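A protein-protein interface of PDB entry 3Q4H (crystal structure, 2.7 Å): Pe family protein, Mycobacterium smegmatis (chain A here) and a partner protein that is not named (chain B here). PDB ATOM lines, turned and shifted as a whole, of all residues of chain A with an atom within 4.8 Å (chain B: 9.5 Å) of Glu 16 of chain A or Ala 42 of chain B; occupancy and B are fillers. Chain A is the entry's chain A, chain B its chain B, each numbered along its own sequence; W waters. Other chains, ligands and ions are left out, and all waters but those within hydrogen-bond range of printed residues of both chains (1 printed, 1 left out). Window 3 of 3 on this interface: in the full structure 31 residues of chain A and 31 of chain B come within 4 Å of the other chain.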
ATOM      1  N   LEU A  12       3.687   5.685  -2.779  1.00  0.00           N
ATOM      2  CA  LEU A  12       4.533   6.804  -3.181  1.00  0.00           C
ATOM      3  C   LEU A  12       5.928   6.689  -2.581  1.00  0.00           C
ATOM      4  O   LEU A  12       6.924   6.748  -3.303  1.00  0.00           O
ATOM      5  CB  LEU A  12       3.896   8.123  -2.754  1.00  0.00           C
ATOM      6  CG  LEU A  12       4.599   9.422  -3.157  1.00  0.00           C
ATOM      7  CD1 LEU A  12       4.776   9.533  -4.683  1.00  0.00           C
ATOM      8  CD2 LEU A  12       3.835  10.636  -2.606  1.00  0.00           C
ATOM      9  N   ILE A  13       5.983   6.533  -1.257  1.00  0.00           N
ATOM     10  CA  ILE A  13       7.232   6.341  -0.517  1.00  0.00           C
ATOM     11  C   ILE A  13       8.045   5.209  -1.124  1.00  0.00           C
ATOM     12  O   ILE A  13       9.250   5.341  -1.317  1.00  0.00           O
ATOM     13  CB  ILE A  13       6.958   5.981   0.961  1.00  0.00           C
ATOM     14  CG1 ILE A  13       6.380   7.178   1.716  1.00  0.00           C
ATOM     15  CG2 ILE A  13       8.230   5.480   1.658  1.00  0.00           C
ATOM     16  CD1 ILE A  13       5.736   6.801   3.024  1.00  0.00           C
ATOM     17  N   ALA A  14       7.378   4.097  -1.417  1.00  0.00           N
ATOM     18  CA  ALA A  14       8.044   2.945  -1.997  1.00  0.00           C
ATOM     19  C   ALA A  14       8.573   3.327  -3.373  1.00  0.00           C
ATOM     20  O   ALA A  14       9.757   3.170  -3.646  1.00  0.00           O
ATOM     21  CB  ALA A  14       7.098   1.761  -2.081  1.00  0.00           C
ATOM     22  N   SER A  15       7.705   3.872  -4.221  1.00  0.00           N
ATOM     23  CA  SER A  15       8.102   4.255  -5.580  1.00  0.00           C
ATOM     24  C   SER A  15       9.313   5.175  -5.592  1.00  0.00           C
ATOM     25  O   SER A  15      10.187   5.039  -6.432  1.00  0.00           O
ATOM     26  CB  SER A  15       6.945   4.936  -6.316  1.00  0.00           C
ATOM     27  OG  SER A  15       5.946   4.000  -6.676  1.00  0.00           O
ATOM     28  N   GLU A  16       9.351   6.115  -4.657  1.00  0.00           N
ATOM     29  CA  GLU A  16      10.415   7.094  -4.623  1.00  0.00           C
ATOM     30  C   GLU A  16      11.690   6.471  -4.081  1.00  0.00           C
ATOM     31  O   GLU A  16      12.776   6.725  -4.613  1.00  0.00           O
ATOM     32  CB  GLU A  16       9.997   8.313  -3.800  1.00  0.00           C
ATOM     33  CG  GLU A  16       8.966   9.196  -4.520  1.00  0.00           C
ATOM     34  CD  GLU A  16       8.500  10.384  -3.698  1.00  0.00           C
ATOM     35  OE1 GLU A  16       8.808  10.449  -2.494  1.00  0.00           O
ATOM     36  OE2 GLU A  16       7.814  11.253  -4.260  1.00  0.00           O
ATOM     37  N   ALA A  17      11.568   5.643  -3.048  1.00  0.00           N
ATOM     38  CA  ALA A  17      12.744   4.997  -2.468  1.00  0.00           C
ATOM     39  C   ALA A  17      13.430   4.137  -3.528  1.00  0.00           C
ATOM     40  O   ALA A  17      14.657   4.192  -3.694  1.00  0.00           O
ATOM     41  CB  ALA A  17      12.372   4.166  -1.232  1.00  0.00           C
ATOM     42  N   ASN A  18      12.626   3.382  -4.272  1.00  0.00           N
ATOM     43  CA  ASN A  18      13.146   2.553  -5.361  1.00  0.00           C
ATOM     44  C   ASN A  18      13.867   3.380  -6.423  1.00  0.00           C
ATOM     45  O   ASN A  18      14.964   3.016  -6.859  1.00  0.00           O
ATOM     46  CB  ASN A  18      12.032   1.689  -5.968  1.00  0.00           C
ATOM     47  CG  ASN A  18      11.547   0.606  -4.999  1.00  0.00           C
ATOM     48  OD1 ASN A  18      12.212   0.311  -4.004  1.00  0.00           O
ATOM     49  ND2 ASN A  18      10.392   0.022  -5.279  1.00  0.00           N
ATOM     50  N   PHE A  19      13.289   4.514  -6.808  1.00  0.00           N
ATOM     51  CA  PHE A  19      14.004   5.436  -7.693  1.00  0.00           C
ATOM     52  C   PHE A  19      15.323   5.875  -7.063  1.00  0.00           C
ATOM     53  O   PHE A  19      16.340   5.964  -7.750  1.00  0.00           O
ATOM     54  CB  PHE A  19      13.174   6.681  -8.042  1.00  0.00           C
ATOM     55  CG  PHE A  19      13.885   7.622  -8.984  1.00  0.00           C
ATOM     56  CD1 PHE A  19      13.799   7.451 -10.356  1.00  0.00           C
ATOM     57  CD2 PHE A  19      14.677   8.652  -8.494  1.00  0.00           C
ATOM     58  CE1 PHE A  19      14.470   8.314 -11.232  1.00  0.00           C
ATOM     59  CE2 PHE A  19      15.354   9.516  -9.369  1.00  0.00           C
ATOM     60  CZ  PHE A  19      15.242   9.346 -10.735  1.00  0.00           C
ATOM     61  N   GLY A  20      15.286   6.155  -5.760  1.00  0.00           N
ATOM     62  CA  GLY A  20      16.469   6.582  -5.028  1.00  0.00           C
ATOM     63  C   GLY A  20      17.567   5.545  -5.039  1.00  0.00           C
ATOM     64  O   GLY A  20      18.739   5.885  -5.118  1.00  0.00           O
ATOM     65  N   ASN A  76      13.465  15.630  -5.464  1.00  0.00           N
ATOM     66  CA  ASN A  76      12.122  15.729  -6.033  1.00  0.00           C
ATOM     67  C   ASN A  76      11.314  14.436  -6.002  1.00  0.00           C
ATOM     68  O   ASN A  76      10.130  14.464  -5.680  1.00  0.00           O
ATOM     69  CB  ASN A  76      12.204  16.235  -7.476  1.00  0.00           C
ATOM     70  CG  ASN A  76      12.316  17.741  -7.556  1.00  0.00           C
ATOM     71  OD1 ASN A  76      11.483  18.459  -7.001  1.00  0.00           O
ATOM     72  ND2 ASN A  76      13.335  18.230  -8.248  1.00  0.00           N
ATOM     73  N   ILE A  77      11.940  13.315  -6.360  1.00  0.00           N
ATOM     74  CA  ILE A  77      11.221  12.039  -6.515  1.00  0.00           C
ATOM     75  C   ILE A  77      12.016  10.819  -6.034  1.00  0.00           C
ATOM     76  O   ILE A  77      11.711   9.693  -6.409  1.00  0.00           O
ATOM     77  CB  ILE A  77      10.803  11.795  -8.003  1.00  0.00           C
ATOM     78  CG1 ILE A  77      12.036  11.763  -8.910  1.00  0.00           C
ATOM     79  CG2 ILE A  77       9.839  12.862  -8.487  1.00  0.00           C
ATOM     80  CD1 ILE A  77      11.761  11.242 -10.307  1.00  0.00           C
ATOM     81  N   GLY A  78      13.017  11.032  -5.186  1.00  0.00           N
ATOM     82  CA  GLY A  78      13.959   9.974  -4.862  1.00  0.00           C
ATOM     83  C   GLY A  78      14.126   9.774  -3.379  1.00  0.00           C
ATOM     84  O   GLY A  78      13.183   9.939  -2.610  1.00  0.00           O
ATOM     85  N   ASP A  79      15.341   9.405  -2.983  1.00  0.00           N
ATOM     86  CA  ASP A  79      15.642   9.060  -1.595  1.00  0.00           C
ATOM     87  C   ASP A  79      15.157  10.102  -0.596  1.00  0.00           C
ATOM     88  O   ASP A  79      14.542   9.748   0.410  1.00  0.00           O
ATOM     89  CB  ASP A  79      17.136   8.842  -1.390  1.00  0.00           C
ATOM     90  CG  ASP A  79      17.433   8.194  -0.064  1.00  0.00           C
ATOM     91  OD1 ASP A  79      17.054   7.019   0.093  1.00  0.00           O
ATOM     92  OD2 ASP A  79      18.022   8.844   0.833  1.00  0.00           O
ATOM     93  N   ALA A  81      13.013  12.739  -1.177  1.00  0.00           N
ATOM     94  CA  ALA A  81      11.582  12.917  -1.295  1.00  0.00           C
ATOM     95  C   ALA A  81      10.861  11.881  -0.427  1.00  0.00           C
ATOM     96  O   ALA A  81      10.035  12.245   0.415  1.00  0.00           O
ATOM     97  CB  ALA A  81      11.153  12.812  -2.740  1.00  0.00           C
ATOM     98  N   SER A  82      11.202  10.605  -0.607  1.00  0.00           N
ATOM     99  CA  SER A  82      10.556   9.517   0.123  1.00  0.00           C
ATOM    100  C   SER A  82      10.699   9.670   1.642  1.00  0.00           C
ATOM    101  O   SER A  82       9.728   9.463   2.386  1.00  0.00           O
ATOM    102  CB  SER A  82      11.135   8.174  -0.298  1.00  0.00           C
ATOM    103  OG  SER A  82      12.476   8.060   0.143  1.00  0.00           O
ATOM    104  N   VAL A  85       8.253  12.400   2.854  1.00  0.00           N
ATOM    105  CA  VAL A  85       6.885  11.876   2.887  1.00  0.00           C
ATOM    106  C   VAL A  85       6.672  10.932   4.061  1.00  0.00           C
ATOM    107  O   VAL A  85       5.619  10.961   4.695  1.00  0.00           O
ATOM    108  CB  VAL A  85       6.517  11.115   1.602  1.00  0.00           C
ATOM    109  CG1 VAL A  85       5.149  10.434   1.766  1.00  0.00           C
ATOM    110  CG2 VAL A  85       6.528  12.052   0.402  1.00  0.00           C
ATOM    111  N   GLU B  35      11.826   5.772 -15.342  1.00  0.00           N
ATOM    112  CA  GLU B  35      11.269   5.894 -13.987  1.00  0.00           C
ATOM    113  C   GLU B  35      10.954   7.341 -13.600  1.00  0.00           C
ATOM    114  O   GLU B  35       9.940   7.600 -12.949  1.00  0.00           O
ATOM    115  CB  GLU B  35      12.195   5.262 -12.934  1.00  0.00           C
ATOM    116  CG  GLU B  35      12.176   3.717 -12.889  1.00  0.00           C
ATOM    117  CD  GLU B  35      11.056   3.132 -12.020  1.00  0.00           C
ATOM    118  OE1 GLU B  35      10.042   3.833 -11.757  1.00  0.00           O
ATOM    119  OE2 GLU B  35      11.191   1.954 -11.605  1.00  0.00           O
ATOM    120  N   GLN B  36      11.813   8.279 -13.993  1.00  0.00           N
ATOM    121  CA  GLN B  36      11.547   9.686 -13.728  1.00  0.00           C
ATOM    122  C   GLN B  36      10.300  10.174 -14.461  1.00  0.00           C
ATOM    123  O   GLN B  36       9.559  11.010 -13.925  1.00  0.00           O
ATOM    124  CB  GLN B  36      12.732  10.572 -14.099  1.00  0.00           C
ATOM    125  CG  GLN B  36      12.581  12.027 -13.605  1.00  0.00           C
ATOM    126  CD  GLN B  36      12.115  13.014 -14.671  1.00  0.00           C
ATOM    127  OE1 GLN B  36      11.968  12.670 -15.844  1.00  0.00           O
ATOM    128  NE2 GLN B  36      11.905  14.263 -14.263  1.00  0.00           N
ATOM    129  N   HIS B  37      10.080   9.673 -15.678  1.00  0.00           N
ATOM    130  CA  HIS B  37       8.863   9.988 -16.416  1.00  0.00           C
ATOM    131  C   HIS B  37       7.645   9.411 -15.698  1.00  0.00           C
ATOM    132  O   HIS B  37       6.668  10.116 -15.469  1.00  0.00           O
ATOM    133  CB  HIS B  37       8.921   9.450 -17.843  1.00  0.00           C
ATOM    134  CG  HIS B  37       7.740   9.840 -18.674  1.00  0.00           C
ATOM    135  ND1 HIS B  37       6.725   8.961 -18.987  1.00  0.00           N
ATOM    136  CD2 HIS B  37       7.393  11.027 -19.229  1.00  0.00           C
ATOM    137  CE1 HIS B  37       5.812   9.584 -19.711  1.00  0.00           C
ATOM    138  NE2 HIS B  37       6.193  10.840 -19.871  1.00  0.00           N
ATOM    139  N   ALA B  38       7.728   8.132 -15.331  1.00  0.00           N
ATOM    140  CA  ALA B  38       6.671   7.447 -14.587  1.00  0.00           C
ATOM    141  C   ALA B  38       6.282   8.168 -13.300  1.00  0.00           C
ATOM    142  O   ALA B  38       5.145   8.063 -12.854  1.00  0.00           O
ATOM    143  CB  ALA B  38       7.091   6.012 -14.277  1.00  0.00           C
ATOM    144  N   LEU B  39       7.225   8.897 -12.709  1.00  0.00           N
ATOM    145  CA  LEU B  39       6.985   9.630 -11.461  1.00  0.00           C
ATOM    146  C   LEU B  39       6.810  11.131 -11.685  1.00  0.00           C
ATOM    147  O   LEU B  39       7.016  11.925 -10.766  1.00  0.00           O
ATOM    148  CB  LEU B  39       8.135   9.391 -10.479  1.00  0.00           C
ATOM    149  CG  LEU B  39       8.145   8.002  -9.848  1.00  0.00           C
ATOM    150  CD1 LEU B  39       9.472   7.734  -9.167  1.00  0.00           C
ATOM    151  CD2 LEU B  39       6.961   7.856  -8.867  1.00  0.00           C
ATOM    152  N   ALA B  40       6.407  11.509 -12.896  1.00  0.00           N
ATOM    153  CA  ALA B  40       6.253  12.915 -13.262  1.00  0.00           C
ATOM    154  C   ALA B  40       5.303  13.662 -12.330  1.00  0.00           C
ATOM    155  O   ALA B  40       5.598  14.786 -11.934  1.00  0.00           O
ATOM    156  CB  ALA B  40       5.776  13.035 -14.704  1.00  0.00           C
ATOM    157  N   SER B  41       4.175  13.041 -11.974  1.00  0.00           N
ATOM    158  CA  SER B  41       3.165  13.699 -11.125  1.00  0.00           C
ATOM    159  C   SER B  41       3.648  14.022  -9.697  1.00  0.00           C
ATOM    160  O   SER B  41       3.088  14.902  -9.036  1.00  0.00           O
ATOM    161  CB  SER B  41       1.875  12.872 -11.065  1.00  0.00           C
ATOM    162  OG  SER B  41       2.111  11.599 -10.508  1.00  0.00           O
ATOM    163  N   ALA B  42       4.683  13.321  -9.232  1.00  0.00           N
ATOM    164  CA  ALA B  42       5.263  13.574  -7.914  1.00  0.00           C
ATOM    165  C   ALA B  42       6.302  14.695  -7.930  1.00  0.00           C
ATOM    166  O   ALA B  42       6.830  15.063  -6.880  1.00  0.00           O
ATOM    167  CB  ALA B  42       5.887  12.296  -7.367  1.00  0.00           C
ATOM    168  N   TRP B  43       6.589  15.230  -9.114  1.00  0.00           N
ATOM    169  CA  TRP B  43       7.648  16.215  -9.300  1.00  0.00           C
ATOM    170  C   TRP B  43       7.140  17.652  -9.174  1.00  0.00           C
ATOM    171  O   TRP B  43       6.131  18.009  -9.779  1.00  0.00           O
ATOM    172  CB  TRP B  43       8.266  16.024 -10.685  1.00  0.00           C
ATOM    173  CG  TRP B  43       9.541  16.769 -10.892  1.00  0.00           C
ATOM    174  CD1 TRP B  43       9.699  18.124 -10.983  1.00  0.00           C
ATOM    175  CD2 TRP B  43      10.843  16.202 -11.059  1.00  0.00           C
ATOM    176  NE1 TRP B  43      11.021  18.434 -11.180  1.00  0.00           N
ATOM    177  CE2 TRP B  43      11.745  17.272 -11.231  1.00  0.00           C
ATOM    178  CE3 TRP B  43      11.337  14.893 -11.072  1.00  0.00           C
ATOM    179  CZ2 TRP B  43      13.113  17.074 -11.416  1.00  0.00           C
ATOM    180  CZ3 TRP B  43      12.696  14.698 -11.252  1.00  0.00           C
ATOM    181  CH2 TRP B  43      13.567  15.782 -11.425  1.00  0.00           C
ATOM    182  N   GLN B  44       7.854  18.472  -8.403  1.00  0.00           N
ATOM    183  CA  GLN B  44       7.641  19.933  -8.385  1.00  0.00           C
ATOM    184  C   GLN B  44       8.983  20.685  -8.580  1.00  0.00           C
ATOM    185  O   GLN B  44      10.050  20.076  -8.621  1.00  0.00           O
ATOM    186  CB  GLN B  44       6.912  20.376  -7.102  1.00  0.00           C
ATOM    187  CG  GLN B  44       7.717  20.274  -5.798  1.00  0.00           C
ATOM    188  CD  GLN B  44       7.821  18.854  -5.255  1.00  0.00           C
ATOM    189  OE1 GLN B  44       8.904  18.272  -5.212  1.00  0.00           O
ATOM    190  NE2 GLN B  44       6.694  18.293  -4.835  1.00  0.00           N
ATOM    191  N   GLY B  45       8.934  22.004  -8.721  1.00  0.00           N
ATOM    192  CA  GLY B  45      10.158  22.792  -8.916  1.00  0.00           C
ATOM    193  C   GLY B  45      10.889  23.062  -7.607  1.00  0.00           C
ATOM    194  O   GLY B  45      10.872  24.199  -7.109  1.00  0.00           O
ATOM    195  N   ASP B  46      11.533  22.026  -7.055  1.00  0.00           N
ATOM    196  CA  ASP B  46      12.222  22.133  -5.751  1.00  0.00           C
ATOM    197  C   ASP B  46      13.402  23.112  -5.824  1.00  0.00           C
ATOM    198  O   ASP B  46      13.369  24.187  -5.205  1.00  0.00           O
ATOM    199  CB  ASP B  46      12.694  20.757  -5.258  1.00  0.00           C
ATOM    200  N   MET B  49      13.779  23.444 -11.060  1.00  0.00           N
ATOM    201  CA  MET B  49      13.835  22.730 -12.334  1.00  0.00           C
ATOM    202  C   MET B  49      12.604  21.851 -12.541  1.00  0.00           C
ATOM    203  O   MET B  49      12.249  21.048 -11.683  1.00  0.00           O
ATOM    204  CB  MET B  49      15.110  21.880 -12.444  1.00  0.00           C
ATOM    205  CG  MET B  49      15.462  21.519 -13.885  1.00  0.00           C
ATOM    206  SD  MET B  49      16.973  20.300 -14.099  1.00  0.00           S
ATOM    207  CE  MET B  49      18.465  21.522 -13.737  1.00  0.00           C
ATOM    208  N   TYR B  51      10.211  18.898 -14.418  1.00  0.00           N
ATOM    209  CA  TYR B  51      10.476  17.501 -14.738  1.00  0.00           C
ATOM    210  C   TYR B  51      10.847  17.333 -16.221  1.00  0.00           C
ATOM    211  O   TYR B  51      11.703  16.520 -16.550  1.00  0.00           O
ATOM    212  CB  TYR B  51       9.301  16.597 -14.307  1.00  0.00           C
ATOM    213  CG  TYR B  51       8.153  16.453 -15.289  1.00  0.00           C
ATOM    214  CD1 TYR B  51       8.241  15.573 -16.375  1.00  0.00           C
ATOM    215  CD2 TYR B  51       6.960  17.161 -15.112  1.00  0.00           C
ATOM    216  CE1 TYR B  51       7.187  15.425 -17.271  1.00  0.00           C
ATOM    217  CE2 TYR B  51       5.898  17.013 -15.998  1.00  0.00           C
ATOM    218  CZ  TYR B  51       6.019  16.142 -17.077  1.00  0.00           C
ATOM    219  OH  TYR B  51       4.974  15.991 -17.964  1.00  0.00           O
HETATM  220  O   HOH W   1       9.808   3.368  -9.009  1.00  0.00           O
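The side-chain amide oxygen (OD1) of Asn 76 of chain A lies close to the backbone carbonyl oxygen (O) of Gln 44 of chain B, at 2.7 Å.
The side-chain carboxylate (OE1) of Glu 16 of chain A lies within hydrogen-bond range of the backbone NH (N) of Ser 82 of chain A (3.1 Å). NE2 of Gln 36 of chain B sits at hydrogen-bond distance from O of Tyr 51 of chain B (3.2 Å). The indole nitrogen (NE1) of Trp 43 of chain B is in hydrogen-bond range of the backbone carbonyl oxygen (O) of Met 49 of chain B (2.9 Å).
Among the printed residues, pairs that only touch across the chains: Asn 76 of chain A with Asp 46 of chain B, Asn 76 of chain A with Trp 43 of chain B, Ile 77 of chain A with Gln 36 of chain B, Asn 76 of chain A with Ala 42 of chain B, Ile 77 of chain A with Trp 43 of chain B, Phe 19 of chain A with Glu 35 of chain B, Ile 77 of chain A with Leu 39 of chain B, Glu 16 of chain A with Ala 42 of chain B, Phe 19 of chain A with Gln 36 of chain B and Ser 15 of chain A with Leu 39 of chain B.
Ser 15 of chain A touches just one residue of chain B: Leu 39 (3.9 Å). Glu 16 of chain A touches just one residue of chain B: Ala 42. No residue of chain B comes within 4 Å of Ala 17 of chain A. Asn 18 of chain A touches none of the printed residues of chain B. Of the printed residues of chain B, Phe 19 of chain A touches Glu 35 and Gln 36. Of the printed residues of chain B, Ile 77 of chain A touches Gln 36 (3.5 Å), Leu 39 (3.7 Å) and Trp 43 (3.6 Å). No residue of chain B comes within 4 Å of Gly 78 of chain A. No residue of chain B comes within 4 Å of Ser 82 of chain A. Printed residues of chain A within 4 Å of Leu 39 of chain B: Ser 15 and Ile 77. Printed residues of chain A within 4 Å of Ala 42 of chain B: Glu 16 (3.8 Å) and Asn 76 (3.6 Å). Of the printed residues of chain A, Gln 44 of chain B touches Asn 76. Printed residues of chain A within 4 Å of Asp 46 of chain B: Asn 76. The nearest residue of chain B that does not touch Glu 16 of chain A is Leu 39 of chain B (4.7 Å).
Along chain A the printed residues that touch a printed residue of chain B span positions 15 to 77. Of the 14 printed residues of chain B, 7 touch a printed residue of chain A. Printed residues of chain B that touch a printed residue of chain A: Glu 35, Gln 36, Leu 39, Ala 42, Trp 43, Gln 44 and Asp 46. Hydrophobic or aromatic side chains of chain B within 4 Å of the printed part of chain A: Leu 39, Ala 42 and Trp 43.
Water W1 lies within hydrogen-bond range of OE1 of Glu 35 of chain B and O of Ser 15 of chain A.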
